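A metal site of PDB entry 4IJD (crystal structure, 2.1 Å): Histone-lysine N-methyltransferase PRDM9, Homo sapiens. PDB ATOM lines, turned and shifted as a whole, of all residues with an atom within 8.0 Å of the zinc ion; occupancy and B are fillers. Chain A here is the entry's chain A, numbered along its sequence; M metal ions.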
ATOM      1  N   TYR A  10     -22.755 -22.496   1.147  1.00  0.00           N
ATOM      2  CA  TYR A  10     -23.770 -21.494   1.360  1.00  0.00           C
ATOM      3  C   TYR A  10     -25.132 -22.149   1.266  1.00  0.00           C
ATOM      4  O   TYR A  10     -25.403 -22.837   0.301  1.00  0.00           O
ATOM      5  CB  TYR A  10     -23.657 -20.426   0.289  1.00  0.00           C
ATOM      6  CG  TYR A  10     -24.553 -19.222   0.511  1.00  0.00           C
ATOM      7  CD1 TYR A  10     -25.701 -19.041  -0.243  1.00  0.00           C
ATOM      8  CD2 TYR A  10     -24.197 -18.242   1.407  1.00  0.00           C
ATOM      9  CE1 TYR A  10     -26.492 -17.916  -0.081  1.00  0.00           C
ATOM     10  CE2 TYR A  10     -24.998 -17.130   1.602  1.00  0.00           C
ATOM     11  CZ  TYR A  10     -26.140 -16.972   0.844  1.00  0.00           C
ATOM     12  OH  TYR A  10     -26.931 -15.847   1.031  1.00  0.00           O
ATOM     13  N   CYS A  11     -25.960 -21.952   2.280  1.00  0.00           N
ATOM     14  CA  CYS A  11     -27.319 -22.440   2.255  1.00  0.00           C
ATOM     15  C   CYS A  11     -28.213 -21.404   1.608  1.00  0.00           C
ATOM     16  O   CYS A  11     -28.359 -20.312   2.118  1.00  0.00           O
ATOM     17  CB  CYS A  11     -27.835 -22.736   3.666  1.00  0.00           C
ATOM     18  SG  CYS A  11     -29.542 -23.336   3.654  1.00  0.00           S
ATOM     19  N   GLU A  12     -28.788 -21.763   0.467  1.00  0.00           N
ATOM     20  CA  GLU A  12     -29.662 -20.864  -0.278  1.00  0.00           C
ATOM     21  C   GLU A  12     -31.016 -20.571   0.435  1.00  0.00           C
ATOM     22  O   GLU A  12     -31.695 -19.614   0.089  1.00  0.00           O
ATOM     23  CB  GLU A  12     -29.905 -21.442  -1.651  1.00  0.00           C
ATOM     24  CG  GLU A  12     -28.706 -21.386  -2.587  1.00  0.00           C
ATOM     25  CD  GLU A  12     -28.405 -19.966  -3.122  1.00  0.00           C
ATOM     26  OE1 GLU A  12     -29.260 -19.059  -2.976  1.00  0.00           O
ATOM     27  OE2 GLU A  12     -27.296 -19.755  -3.667  1.00  0.00           O
ATOM     28  N   MET A  13     -31.393 -21.379   1.420  1.00  0.00           N
ATOM     29  CA  MET A  13     -32.631 -21.116   2.183  1.00  0.00           C
ATOM     30  C   MET A  13     -32.383 -20.173   3.319  1.00  0.00           C
ATOM     31  O   MET A  13     -33.118 -19.196   3.475  1.00  0.00           O
ATOM     32  CB  MET A  13     -33.241 -22.374   2.742  1.00  0.00           C
ATOM     33  CG  MET A  13     -34.214 -22.985   1.739  1.00  0.00           C
ATOM     34  SD  MET A  13     -34.095 -24.934   1.876  1.00  0.00           S
ATOM     35  CE  MET A  13     -32.316 -25.142   1.026  1.00  0.00           C
ATOM     36  N   CYS A  14     -31.358 -20.454   4.129  1.00  0.00           N
ATOM     37  CA  CYS A  14     -30.948 -19.532   5.173  1.00  0.00           C
ATOM     38  C   CYS A  14     -30.327 -18.263   4.558  1.00  0.00           C
ATOM     39  O   CYS A  14     -30.410 -17.195   5.130  1.00  0.00           O
ATOM     40  CB  CYS A  14     -29.940 -20.189   6.115  1.00  0.00           C
ATOM     41  SG  CYS A  14     -30.593 -21.633   6.988  1.00  0.00           S
ATOM     42  N   GLN A  15     -29.734 -18.383   3.377  1.00  0.00           N
ATOM     43  CA  GLN A  15     -28.894 -17.318   2.830  1.00  0.00           C
ATOM     44  C   GLN A  15     -27.742 -17.047   3.812  1.00  0.00           C
ATOM     45  O   GLN A  15     -27.567 -15.937   4.310  1.00  0.00           O
ATOM     46  CB  GLN A  15     -29.709 -16.018   2.547  1.00  0.00           C
ATOM     47  CG  GLN A  15     -30.684 -16.102   1.371  1.00  0.00           C
ATOM     48  CD  GLN A  15     -29.989 -16.190  -0.004  1.00  0.00           C
ATOM     49  OE1 GLN A  15     -28.944 -15.553  -0.265  1.00  0.00           O
ATOM     50  NE2 GLN A  15     -30.573 -16.948  -0.904  1.00  0.00           N
ATOM     51  N   ASN A  16     -27.023 -18.101   4.167  1.00  0.00           N
ATOM     52  CA  ASN A  16     -25.812 -17.934   4.938  1.00  0.00           C
ATOM     53  C   ASN A  16     -24.914 -19.145   4.842  1.00  0.00           C
ATOM     54  O   ASN A  16     -25.313 -20.180   4.309  1.00  0.00           O
ATOM     55  CB  ASN A  16     -26.077 -17.528   6.395  1.00  0.00           C
ATOM     56  CG  ASN A  16     -26.658 -18.662   7.248  1.00  0.00           C
ATOM     57  OD1 ASN A  16     -26.209 -19.806   7.183  1.00  0.00           O
ATOM     58  ND2 ASN A  16     -27.611 -18.315   8.096  1.00  0.00           N
ATOM     59  N   PHE A  17     -23.697 -18.971   5.331  1.00  0.00           N
ATOM     60  CA  PHE A  17     -22.630 -19.913   5.094  1.00  0.00           C
ATOM     61  C   PHE A  17     -22.656 -20.968   6.162  1.00  0.00           C
ATOM     62  O   PHE A  17     -23.138 -20.702   7.245  1.00  0.00           O
ATOM     63  CB  PHE A  17     -21.284 -19.188   5.101  1.00  0.00           C
ATOM     64  CG  PHE A  17     -21.066 -18.338   3.885  1.00  0.00           C
ATOM     65  CD1 PHE A  17     -20.696 -18.918   2.683  1.00  0.00           C
ATOM     66  CD2 PHE A  17     -21.251 -16.964   3.933  1.00  0.00           C
ATOM     67  CE1 PHE A  17     -20.509 -18.139   1.545  1.00  0.00           C
ATOM     68  CE2 PHE A  17     -21.057 -16.180   2.798  1.00  0.00           C
ATOM     69  CZ  PHE A  17     -20.704 -16.778   1.600  1.00  0.00           C
ATOM     70  N   PHE A  18     -22.143 -22.158   5.853  1.00  0.00           N
ATOM     71  CA  PHE A  18     -21.950 -23.220   6.879  1.00  0.00           C
ATOM     72  C   PHE A  18     -20.779 -24.138   6.525  1.00  0.00           C
ATOM     73  O   PHE A  18     -20.291 -24.113   5.392  1.00  0.00           O
ATOM     74  CB  PHE A  18     -23.217 -24.068   7.012  1.00  0.00           C
ATOM     75  CG  PHE A  18     -23.636 -24.790   5.726  1.00  0.00           C
ATOM     76  CD1 PHE A  18     -24.422 -24.156   4.783  1.00  0.00           C
ATOM     77  CD2 PHE A  18     -23.280 -26.114   5.505  1.00  0.00           C
ATOM     78  CE1 PHE A  18     -24.838 -24.834   3.628  1.00  0.00           C
ATOM     79  CE2 PHE A  18     -23.669 -26.784   4.367  1.00  0.00           C
ATOM     80  CZ  PHE A  18     -24.447 -26.138   3.416  1.00  0.00           C
ATOM     81  N   SER A  21     -22.630 -29.346   7.081  1.00  0.00           N
ATOM     82  CA  SER A  21     -24.088 -29.353   6.924  1.00  0.00           C
ATOM     83  C   SER A  21     -24.775 -28.169   7.618  1.00  0.00           C
ATOM     84  O   SER A  21     -24.317 -27.699   8.632  1.00  0.00           O
ATOM     85  CB  SER A  21     -24.670 -30.663   7.426  1.00  0.00           C
ATOM     86  OG  SER A  21     -24.574 -30.682   8.795  1.00  0.00           O
ATOM     87  N   CYS A  22     -25.886 -27.705   7.035  1.00  0.00           N
ATOM     88  CA  CYS A  22     -26.628 -26.557   7.562  1.00  0.00           C
ATOM     89  C   CYS A  22     -27.387 -26.993   8.790  1.00  0.00           C
ATOM     90  O   CYS A  22     -28.107 -27.995   8.779  1.00  0.00           O
ATOM     91  CB  CYS A  22     -27.619 -25.979   6.547  1.00  0.00           C
ATOM     92  SG  CYS A  22     -28.650 -24.696   7.290  1.00  0.00           S
ATOM     93  N   ALA A  23     -27.181 -26.252   9.873  1.00  0.00           N
ATOM     94  CA  ALA A  23     -27.853 -26.535  11.135  1.00  0.00           C
ATOM     95  C   ALA A  23     -29.395 -26.564  11.009  1.00  0.00           C
ATOM     96  O   ALA A  23     -30.054 -27.275  11.741  1.00  0.00           O
ATOM     97  CB  ALA A  23     -27.431 -25.522  12.183  1.00  0.00           C
ATOM     98  N   ALA A  24     -29.952 -25.786  10.077  1.00  0.00           N
ATOM     99  CA  ALA A  24     -31.408 -25.721   9.919  1.00  0.00           C
ATOM    100  C   ALA A  24     -31.916 -26.741   8.911  1.00  0.00           C
ATOM    101  O   ALA A  24     -33.017 -27.276   9.090  1.00  0.00           O
ATOM    102  CB  ALA A  24     -31.844 -24.325   9.514  1.00  0.00           C
ATOM    103  N   HIS A  25     -31.120 -27.011   7.876  1.00  0.00           N
ATOM    104  CA  HIS A  25     -31.577 -27.802   6.725  1.00  0.00           C
ATOM    105  C   HIS A  25     -30.829 -29.091   6.465  1.00  0.00           C
ATOM    106  O   HIS A  25     -31.195 -29.864   5.584  1.00  0.00           O
ATOM    107  CB  HIS A  25     -31.555 -26.929   5.490  1.00  0.00           C
ATOM    108  CG  HIS A  25     -32.476 -25.733   5.598  1.00  0.00           C
ATOM    109  ND1 HIS A  25     -32.037 -24.497   5.849  1.00  0.00           N
ATOM    110  CD2 HIS A  25     -33.863 -25.650   5.510  1.00  0.00           C
ATOM    111  CE1 HIS A  25     -33.081 -23.656   5.911  1.00  0.00           C
ATOM    112  NE2 HIS A  25     -34.198 -24.361   5.715  1.00  0.00           N
ATOM    113  N   GLY A  26     -29.767 -29.352   7.234  1.00  0.00           N
ATOM    114  CA  GLY A  26     -28.996 -30.574   7.064  1.00  0.00           C
ATOM    115  C   GLY A  26     -27.989 -30.504   5.941  1.00  0.00           C
ATOM    116  O   GLY A  26     -27.682 -29.421   5.449  1.00  0.00           O
HETATM  117 ZN    ZN M   1     -30.070 -23.615   5.832  1.00  0.00          ZN
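Of the 15 residues printed, 4 come within 4 Å of the zinc ion.
The nearest printed residue that does not touch the zinc ion is Ala 24 (4.1 Å).
N of Met 13 lies close to SG of Cys 11 (3.5 Å).
N of Cys 11 lies within hydrogen-bond range of O of Asn 16 (2.8 Å).
SG of Cys 22 sits close to N of Ala 24.
The zinc ion is bound by ND1 of His 25 (2.2 Å), SG of Cys 11 (2.3 Å), SG of Cys 22 (2.3 Å) and SG of Cys 14 (2.4 Å).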
